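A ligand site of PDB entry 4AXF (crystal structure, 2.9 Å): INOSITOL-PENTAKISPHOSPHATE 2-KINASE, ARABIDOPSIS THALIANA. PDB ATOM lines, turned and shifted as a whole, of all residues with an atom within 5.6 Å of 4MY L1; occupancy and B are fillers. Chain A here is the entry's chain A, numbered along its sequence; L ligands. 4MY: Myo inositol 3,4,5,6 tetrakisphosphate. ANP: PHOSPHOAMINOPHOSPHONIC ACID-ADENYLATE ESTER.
The guanidinium group of Arg 50 lies within salt-bridge range of an oxygen (O33) of 4MY L1 (2.6 Å).
The side-chain hydroxyl (OH) of Tyr 424 lies within hydrogen-bond range of an oxygen (O24) of 4MY L1, at 2.7 Å.
NH1 of Arg 420 is in salt-bridge range of O24 of 4MY L1 (2.8 Å).
The side-chain amino group (NZ) of Lys 205 is in salt-bridge range of an oxygen (O46) of 4MY L1 (2.8 Å).
The side-chain amino group (NZ) of Lys 175 is in salt-bridge range of an oxygen (O36) of 4MY L1 (2.8 Å).
The side-chain carboxylate of Asp 373 lies within hydrogen-bond range of an oxygen (O12) of 4MY L1 (3.2 Å).
An oxygen (O26) of 4MY L1 sits close to the side-chain amide oxygen (OD1) of Asn 243 (2.9 Å).
An oxygen (O43) of 4MY L1 is in salt-bridge range of the side-chain amino group of Lys 416, 3.2 Å away.
The backbone NH (N) of Gly 25 sits close to an oxygen (O23) of 4MY L1, 3.3 Å away.
N of Ala 26 sits at hydrogen-bond distance from O23 of 4MY L1 (3.3 Å).
NZ of Lys 173 lies within salt-bridge range of O36 of 4MY L1 (3.7 Å).
The side-chain carboxylate of Asp 373 lies close to an oxygen (O2G) of ANP L2, at 2.7 Å.
The backbone NH of Gly 25 sits at hydrogen-bond distance from an oxygen (O3G) of ANP L2 (2.6 Å).
The backbone NH (N) of Ala 26 is in hydrogen-bond range of an oxygen (O1B) of ANP L2, at 3.0 Å.
An oxygen (O2G) of ANP L2 lies within salt-bridge range of the side-chain amino group of Lys 173, at 3.2 Å.
The backbone NH (N) of Gly 24 lies close to an oxygen (O1B) of ANP L2.
A nitrogen (N3B) of ANP L2 sits at hydrogen-bond distance from the side-chain carboxylate of Asp 412 (3.1 Å).
O3G of ANP L2 lies within hydrogen-bond range of O12 of 4MY L1, 2.7 Å away.
OD1 of Asp 373 is in salt-bridge range of NZ of Lys 175 (3.2 Å).
The side-chain carboxylate (OD2) of Asp 373 is in salt-bridge range of the side-chain amino group (NZ) of Lys 416.
The side-chain carboxylate (OD1) of Asp 373 lies within salt-bridge range of the side-chain amino group (NZ) of Lys 173 (2.6 Å).
ND2 of Asn 243 lies within hydrogen-bond range of OD1 of Asn 244 (3.1 Å).
The backbone NH (N) of Lys 173 sits at hydrogen-bond distance from the backbone carbonyl oxygen (O) of Asn 244.
Residues that only touch 4MY L1: His 201 and Leu 427.
Hydrophobic or aromatic side chains that line 4MY L1: Ala 26, His 201, Tyr 424 and Leu 427.
Of the 19 residues printed, 13 come within 4 Å of 4MY L1.
The nearest printed residue that does not touch 4MY L1 is Ala 369 (4.4 Å).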
ATOM      1  N   GLY A  24      -0.286  10.639 -26.953  1.00  0.00           N
ATOM      2  CA  GLY A  24      -0.685   9.289 -27.297  1.00  0.00           C
ATOM      3  C   GLY A  24      -2.059   9.348 -27.938  1.00  0.00           C
ATOM      4  O   GLY A  24      -2.327  10.246 -28.745  1.00  0.00           O
ATOM      5  N   GLY A  25      -2.932   8.425 -27.563  1.00  0.00           N
ATOM      6  CA  GLY A  25      -4.275   8.383 -28.131  1.00  0.00           C
ATOM      7  C   GLY A  25      -5.352   8.947 -27.210  1.00  0.00           C
ATOM      8  O   GLY A  25      -6.520   8.986 -27.586  1.00  0.00           O
ATOM      9  N   ALA A  26      -4.950   9.382 -26.021  1.00  0.00           N
ATOM     10  CA  ALA A  26      -5.904   9.871 -25.029  1.00  0.00           C
ATOM     11  C   ALA A  26      -5.568  11.281 -24.536  1.00  0.00           C
ATOM     12  O   ALA A  26      -6.458  12.081 -24.248  1.00  0.00           O
ATOM     13  CB  ALA A  26      -5.982   8.909 -23.863  1.00  0.00           C
ATOM     14  N   ARG A  50     -12.155  12.171 -29.114  1.00  0.00           N
ATOM     15  CA  ARG A  50     -12.000  11.456 -30.372  1.00  0.00           C
ATOM     16  C   ARG A  50     -13.057  11.909 -31.378  1.00  0.00           C
ATOM     17  O   ARG A  50     -13.980  12.654 -31.022  1.00  0.00           O
ATOM     18  CB  ARG A  50     -12.060   9.932 -30.150  1.00  0.00           C
ATOM     19  CG  ARG A  50     -10.944   9.410 -29.245  1.00  0.00           C
ATOM     20  CD  ARG A  50     -10.957   7.893 -29.107  1.00  0.00           C
ATOM     21  NE  ARG A  50      -9.744   7.426 -28.446  1.00  0.00           N
ATOM     22  CZ  ARG A  50      -9.356   6.150 -28.361  1.00  0.00           C
ATOM     23  NH1 ARG A  50     -10.090   5.181 -28.908  1.00  0.00           N
ATOM     24  NH2 ARG A  50      -8.225   5.850 -27.742  1.00  0.00           N
ATOM     25  N   ARG A 135      -2.640  11.945 -36.412  1.00  0.00           N
ATOM     26  CA  ARG A 135      -3.061  12.270 -35.045  1.00  0.00           C
ATOM     27  C   ARG A 135      -4.081  13.403 -35.067  1.00  0.00           C
ATOM     28  O   ARG A 135      -5.076  13.350 -34.335  1.00  0.00           O
ATOM     29  CB  ARG A 135      -1.852  12.661 -34.185  1.00  0.00           C
ATOM     30  CG  ARG A 135      -1.015  11.485 -33.712  1.00  0.00           C
ATOM     31  CD  ARG A 135      -1.762  10.630 -32.698  1.00  0.00           C
ATOM     32  NE  ARG A 135      -0.842   9.751 -31.958  1.00  0.00           N
ATOM     33  CZ  ARG A 135      -1.220   8.715 -31.220  1.00  0.00           C
ATOM     34  NH1 ARG A 135      -2.504   8.394 -31.108  1.00  0.00           N
ATOM     35  NH2 ARG A 135      -0.311   7.995 -30.587  1.00  0.00           N
ATOM     36  N   LYS A 173       8.374   2.636 -23.616  1.00  0.00           N
ATOM     37  CA  LYS A 173       7.042   2.022 -23.590  1.00  0.00           C
ATOM     38  C   LYS A 173       7.226   0.506 -23.780  1.00  0.00           C
ATOM     39  O   LYS A 173       7.274   0.019 -24.909  1.00  0.00           O
ATOM     40  CB  LYS A 173       6.175   2.631 -24.699  1.00  0.00           C
ATOM     41  CG  LYS A 173       4.683   2.337 -24.599  1.00  0.00           C
ATOM     42  CD  LYS A 173       3.936   3.275 -25.539  1.00  0.00           C
ATOM     43  CE  LYS A 173       2.690   2.646 -26.140  1.00  0.00           C
ATOM     44  NZ  LYS A 173       1.449   2.948 -25.385  1.00  0.00           N
ATOM     45  N   LYS A 175       5.508  -2.281 -23.208  1.00  0.00           N
ATOM     46  CA  LYS A 175       4.392  -3.164 -23.589  1.00  0.00           C
ATOM     47  C   LYS A 175       4.345  -4.443 -22.748  1.00  0.00           C
ATOM     48  O   LYS A 175       4.907  -4.486 -21.651  1.00  0.00           O
ATOM     49  CB  LYS A 175       4.383  -3.449 -25.100  1.00  0.00           C
ATOM     50  CG  LYS A 175       4.209  -2.211 -25.967  1.00  0.00           C
ATOM     51  CD  LYS A 175       2.920  -1.449 -25.670  1.00  0.00           C
ATOM     52  CE  LYS A 175       1.683  -2.136 -26.237  1.00  0.00           C
ATOM     53  NZ  LYS A 175       0.495  -1.241 -26.236  1.00  0.00           N
ATOM     54  N   ARG A 197       2.644 -10.896 -28.059  1.00  0.00           N
ATOM     55  CA  ARG A 197       1.642 -10.042 -28.673  1.00  0.00           C
ATOM     56  C   ARG A 197       2.311  -8.913 -29.461  1.00  0.00           C
ATOM     57  O   ARG A 197       1.857  -8.558 -30.552  1.00  0.00           O
ATOM     58  CB  ARG A 197       0.691  -9.496 -27.590  1.00  0.00           C
ATOM     59  CG  ARG A 197      -0.157  -8.300 -27.991  1.00  0.00           C
ATOM     60  CD  ARG A 197      -1.276  -8.664 -28.955  1.00  0.00           C
ATOM     61  NE  ARG A 197      -2.323  -7.656 -28.932  1.00  0.00           N
ATOM     62  CZ  ARG A 197      -3.554  -7.855 -28.460  1.00  0.00           C
ATOM     63  NH1 ARG A 197      -3.918  -9.042 -27.990  1.00  0.00           N
ATOM     64  NH2 ARG A 197      -4.445  -6.865 -28.486  1.00  0.00           N
ATOM     65  N   HIS A 201       1.776  -8.170 -33.393  1.00  0.00           N
ATOM     66  CA  HIS A 201       1.133  -6.914 -33.734  1.00  0.00           C
ATOM     67  C   HIS A 201       1.893  -6.167 -34.803  1.00  0.00           C
ATOM     68  O   HIS A 201       1.277  -5.486 -35.631  1.00  0.00           O
ATOM     69  CB  HIS A 201       0.970  -6.034 -32.503  1.00  0.00           C
ATOM     70  CG  HIS A 201      -0.192  -5.061 -32.578  1.00  0.00           C
ATOM     71  ND1 HIS A 201      -0.838  -4.614 -31.489  1.00  0.00           N
ATOM     72  CD2 HIS A 201      -0.831  -4.480 -33.685  1.00  0.00           C
ATOM     73  CE1 HIS A 201      -1.824  -3.780 -31.863  1.00  0.00           C
ATOM     74  NE2 HIS A 201      -1.821  -3.693 -33.202  1.00  0.00           N
ATOM     75  N   LYS A 205       0.508  -4.134 -37.974  1.00  0.00           N
ATOM     76  CA  LYS A 205       0.812  -2.708 -38.029  1.00  0.00           C
ATOM     77  C   LYS A 205       1.415  -2.350 -39.393  1.00  0.00           C
ATOM     78  O   LYS A 205       0.985  -1.390 -40.027  1.00  0.00           O
ATOM     79  CB  LYS A 205       1.776  -2.310 -36.914  1.00  0.00           C
ATOM     80  CG  LYS A 205       1.161  -2.252 -35.533  1.00  0.00           C
ATOM     81  CD  LYS A 205       2.238  -2.146 -34.479  1.00  0.00           C
ATOM     82  CE  LYS A 205       1.655  -1.970 -33.083  1.00  0.00           C
ATOM     83  NZ  LYS A 205       1.121  -0.594 -32.873  1.00  0.00           N
ATOM     84  N   ASN A 243       7.445   3.749 -31.375  1.00  0.00           N
ATOM     85  CA  ASN A 243       6.773   4.486 -30.308  1.00  0.00           C
ATOM     86  C   ASN A 243       7.131   3.962 -28.908  1.00  0.00           C
ATOM     87  O   ASN A 243       6.425   4.245 -27.929  1.00  0.00           O
ATOM     88  CB  ASN A 243       5.256   4.547 -30.552  1.00  0.00           C
ATOM     89  CG  ASN A 243       4.543   3.224 -30.307  1.00  0.00           C
ATOM     90  OD1 ASN A 243       3.356   3.204 -29.996  1.00  0.00           O
ATOM     91  ND2 ASN A 243       5.264   2.101 -30.448  1.00  0.00           N
ATOM     92  N   ASN A 244       8.236   3.218 -28.830  1.00  0.00           N
ATOM     93  CA  ASN A 244       8.638   2.495 -27.615  1.00  0.00           C
ATOM     94  C   ASN A 244       9.915   3.012 -26.949  1.00  0.00           C
ATOM     95  O   ASN A 244      10.210   2.651 -25.812  1.00  0.00           O
ATOM     96  CB  ASN A 244       8.794   0.993 -27.925  1.00  0.00           C
ATOM     97  CG  ASN A 244       7.559   0.397 -28.588  1.00  0.00           C
ATOM     98  OD1 ASN A 244       7.570   0.110 -29.783  1.00  0.00           O
ATOM     99  ND2 ASN A 244       6.501   0.212 -27.812  1.00  0.00           N
ATOM    100  N   ALA A 369      -4.274  -3.871 -18.361  1.00  0.00           N
ATOM    101  CA  ALA A 369      -4.201  -3.092 -19.598  1.00  0.00           C
ATOM    102  C   ALA A 369      -3.520  -1.744 -19.392  1.00  0.00           C
ATOM    103  O   ALA A 369      -2.781  -1.277 -20.251  1.00  0.00           O
ATOM    104  CB  ALA A 369      -5.592  -2.908 -20.184  1.00  0.00           C
ATOM    105  N   ASP A 373       0.219  -0.660 -21.054  1.00  0.00           N
ATOM    106  CA  ASP A 373       0.267   0.525 -21.908  1.00  0.00           C
ATOM    107  C   ASP A 373       0.976   1.754 -21.328  1.00  0.00           C
ATOM    108  O   ASP A 373       1.053   2.794 -21.983  1.00  0.00           O
ATOM    109  CB  ASP A 373      -1.144   0.903 -22.377  1.00  0.00           C
ATOM    110  CG  ASP A 373      -1.117   1.732 -23.649  1.00  0.00           C
ATOM    111  OD1 ASP A 373      -0.471   1.312 -24.628  1.00  0.00           O
ATOM    112  OD2 ASP A 373      -1.759   2.811 -23.668  1.00  0.00           O
ATOM    113  N   ASP A 412       1.766   7.792 -17.860  1.00  0.00           N
ATOM    114  CA  ASP A 412       0.712   7.263 -18.733  1.00  0.00           C
ATOM    115  C   ASP A 412      -0.050   6.098 -18.068  1.00  0.00           C
ATOM    116  O   ASP A 412      -0.184   5.006 -18.637  1.00  0.00           O
ATOM    117  CB  ASP A 412       1.315   6.853 -20.089  1.00  0.00           C
ATOM    118  CG  ASP A 412       0.271   6.436 -21.113  1.00  0.00           C
ATOM    119  OD1 ASP A 412      -0.925   6.765 -20.962  1.00  0.00           O
ATOM    120  OD2 ASP A 412       0.672   5.756 -22.087  1.00  0.00           O
ATOM    121  N   LYS A 416      -8.658   2.445 -18.459  1.00  0.00           N
ATOM    122  CA  LYS A 416      -9.247   1.929 -19.692  1.00  0.00           C
ATOM    123  C   LYS A 416     -10.757   1.711 -19.504  1.00  0.00           C
ATOM    124  O   LYS A 416     -11.162   1.102 -18.512  1.00  0.00           O
ATOM    125  CB  LYS A 416      -8.556   0.634 -20.132  1.00  0.00           C
ATOM    126  CG  LYS A 416      -7.025   0.706 -20.195  1.00  0.00           C
ATOM    127  CD  LYS A 416      -6.543   1.699 -21.247  1.00  0.00           C
ATOM    128  CE  LYS A 416      -5.046   1.961 -21.124  1.00  0.00           C
ATOM    129  NZ  LYS A 416      -4.539   2.936 -22.136  1.00  0.00           N
ATOM    130  N   ARG A 420     -14.434  -1.143 -23.738  1.00  0.00           N
ATOM    131  CA  ARG A 420     -13.296  -1.458 -24.609  1.00  0.00           C
ATOM    132  C   ARG A 420     -12.901  -2.950 -24.623  1.00  0.00           C
ATOM    133  O   ARG A 420     -12.032  -3.349 -25.396  1.00  0.00           O
ATOM    134  CB  ARG A 420     -12.097  -0.574 -24.254  1.00  0.00           C
ATOM    135  CG  ARG A 420     -11.018  -0.485 -25.328  1.00  0.00           C
ATOM    136  CD  ARG A 420      -9.842   0.368 -24.878  1.00  0.00           C
ATOM    137  NE  ARG A 420     -10.072   1.789 -25.123  1.00  0.00           N
ATOM    138  CZ  ARG A 420      -9.197   2.752 -24.844  1.00  0.00           C
ATOM    139  NH1 ARG A 420      -8.028   2.462 -24.289  1.00  0.00           N
ATOM    140  NH2 ARG A 420      -9.491   4.017 -25.112  1.00  0.00           N
ATOM    141  N   TYR A 424     -11.163  -4.996 -27.588  1.00  0.00           N
ATOM    142  CA  TYR A 424      -9.984  -5.795 -27.230  1.00  0.00           C
ATOM    143  C   TYR A 424     -10.025  -7.191 -27.856  1.00  0.00           C
ATOM    144  O   TYR A 424      -9.014  -7.678 -28.352  1.00  0.00           O
ATOM    145  CB  TYR A 424      -9.800  -5.915 -25.717  1.00  0.00           C
ATOM    146  CG  TYR A 424      -9.180  -4.714 -25.034  1.00  0.00           C
ATOM    147  CD1 TYR A 424      -8.242  -3.913 -25.707  1.00  0.00           C
ATOM    148  CD2 TYR A 424      -9.527  -4.372 -23.730  1.00  0.00           C
ATOM    149  CE1 TYR A 424      -7.672  -2.816 -25.085  1.00  0.00           C
ATOM    150  CE2 TYR A 424      -8.957  -3.263 -23.100  1.00  0.00           C
ATOM    151  CZ  TYR A 424      -8.031  -2.488 -23.785  1.00  0.00           C
ATOM    152  OH  TYR A 424      -7.461  -1.402 -23.170  1.00  0.00           O
ATOM    153  N   LEU A 427      -9.647  -6.877 -31.780  1.00  0.00           N
ATOM    154  CA  LEU A 427      -8.266  -6.584 -32.128  1.00  0.00           C
ATOM    155  C   LEU A 427      -7.386  -7.815 -31.975  1.00  0.00           C
ATOM    156  O   LEU A 427      -6.539  -8.093 -32.824  1.00  0.00           O
ATOM    157  CB  LEU A 427      -7.722  -5.401 -31.317  1.00  0.00           C
ATOM    158  CG  LEU A 427      -6.290  -4.944 -31.629  1.00  0.00           C
ATOM    159  CD1 LEU A 427      -6.165  -4.363 -33.027  1.00  0.00           C
ATOM    160  CD2 LEU A 427      -5.785  -3.946 -30.599  1.00  0.00           C
HETATM  161  C1  4MY L   1      -1.989   3.042 -28.844  1.00  0.00           C
HETATM  162  C2  4MY L   1      -2.561   3.793 -27.648  1.00  0.00           C
HETATM  163  C3  4MY L   1      -3.771   3.041 -27.070  1.00  0.00           C
HETATM  164  P3  4MY L   1      -5.379   4.742 -25.817  1.00  0.00           P
HETATM  165  C4  4MY L   1      -3.454   1.579 -26.752  1.00  0.00           C
HETATM  166  P4  4MY L   1      -4.821   0.021 -25.073  1.00  0.00           P
HETATM  167  C5  4MY L   1      -2.771   0.822 -27.890  1.00  0.00           C
HETATM  168  P5  4MY L   1      -2.585  -1.846 -28.089  1.00  0.00           P
HETATM  169  C6  4MY L   1      -1.581   1.604 -28.463  1.00  0.00           C
HETATM  170  P6  4MY L   1       0.537   0.492 -29.689  1.00  0.00           P
HETATM  171  O11 4MY L   1      -0.878   3.766 -29.393  1.00  0.00           O
HETATM  172  O12 4MY L   1      -1.565   3.952 -26.622  1.00  0.00           O
HETATM  173  O13 4MY L   1      -4.185   3.660 -25.857  1.00  0.00           O
HETATM  174  O14 4MY L   1      -4.684   0.952 -26.381  1.00  0.00           O
HETATM  175  O15 4MY L   1      -2.289  -0.425 -27.387  1.00  0.00           O
HETATM  176  O16 4MY L   1      -1.028   0.919 -29.579  1.00  0.00           O
HETATM  177  O23 4MY L   1      -4.651   6.050 -26.001  1.00  0.00           O
HETATM  178  O24 4MY L   1      -6.064   0.512 -24.357  1.00  0.00           O
HETATM  179  O25 4MY L   1      -1.925  -1.788 -29.440  1.00  0.00           O
HETATM  180  O26 4MY L   1       1.094   1.477 -30.704  1.00  0.00           O
HETATM  181  O33 4MY L   1      -6.298   4.354 -26.971  1.00  0.00           O
HETATM  182  O34 4MY L   1      -3.556   0.273 -24.297  1.00  0.00           O
HETATM  183  O35 4MY L   1      -1.916  -2.825 -27.140  1.00  0.00           O
HETATM  184  O36 4MY L   1       1.119   0.619 -28.302  1.00  0.00           O
HETATM  185  O43 4MY L   1      -5.990   4.577 -24.434  1.00  0.00           O
HETATM  186  O44 4MY L   1      -4.929  -1.373 -25.627  1.00  0.00           O
HETATM  187  O45 4MY L   1      -4.088  -1.932 -28.181  1.00  0.00           O
HETATM  188  O46 4MY L   1       0.482  -0.922 -30.190  1.00  0.00           O
HETATM  189  PG  ANP L   2      -1.585   6.346 -24.562  1.00  0.00           P
HETATM  190  O1G ANP L   2      -2.830   6.331 -23.683  1.00  0.00           O
HETATM  191  O2G ANP L   2      -0.660   5.165 -24.331  1.00  0.00           O
HETATM  192  O3G ANP L   2      -1.844   6.580 -26.039  1.00  0.00           O
HETATM  193  PB  ANP L   2      -1.498   9.245 -23.539  1.00  0.00           P
HETATM  194  O1B ANP L   2      -2.249   9.798 -24.729  1.00  0.00           O
HETATM  195  O2B ANP L   2      -2.287   8.973 -22.287  1.00  0.00           O
HETATM  196  N3B ANP L   2      -0.684   7.764 -24.009  1.00  0.00           N
HETATM  197  PA  ANP L   2       0.959  10.010 -22.267  1.00  0.00           P
HETATM  198  O1A ANP L   2       1.618   8.733 -22.770  1.00  0.00           O
HETATM  199  O2A ANP L   2       0.593  10.138 -20.800  1.00  0.00           O
HETATM  200  O3A ANP L   2      -0.365  10.333 -23.155  1.00  0.00           O
HETATM  201  O5' ANP L   2       1.929  11.232 -22.653  1.00  0.00           O
HETATM  202  C5' ANP L   2       2.293  11.438 -24.019  1.00  0.00           C
HETATM  203  C4' ANP L   2       3.770  11.789 -24.126  1.00  0.00           C
HETATM  204  O4' ANP L   2       4.055  12.976 -23.382  1.00  0.00           O
HETATM  205  C3' ANP L   2       4.654  10.699 -23.565  1.00  0.00           C
HETATM  206  O3' ANP L   2       5.097   9.817 -24.594  1.00  0.00           O
HETATM  207  C2' ANP L   2       5.809  11.455 -22.924  1.00  0.00           C
HETATM  208  O2' ANP L   2       6.910  11.581 -23.839  1.00  0.00           O
HETATM  209  C1' ANP L   2       5.270  12.846 -22.648  1.00  0.00           C
HETATM  210  N9  ANP L   2       5.044  12.998 -21.181  1.00  0.00           N
HETATM  211  C8  ANP L   2       3.904  12.709 -20.516  1.00  0.00           C
HETATM  212  N7  ANP L   2       4.021  12.955 -19.188  1.00  0.00           N
HETATM  213  C5  ANP L   2       5.273  13.417 -18.979  1.00  0.00           C
HETATM  214  C6  ANP L   2       6.072  13.867 -17.802  1.00  0.00           C
HETATM  215  N6  ANP L   2       5.539  13.886 -16.565  1.00  0.00           N
HETATM  216  N1  ANP L   2       7.354  14.272 -18.025  1.00  0.00           N
HETATM  217  C2  ANP L   2       7.896  14.272 -19.266  1.00  0.00           C
HETATM  218  N3  ANP L   2       7.232  13.874 -20.369  1.00  0.00           N
HETATM  219  C4  ANP L   2       5.952  13.436 -20.299  1.00  0.00           C
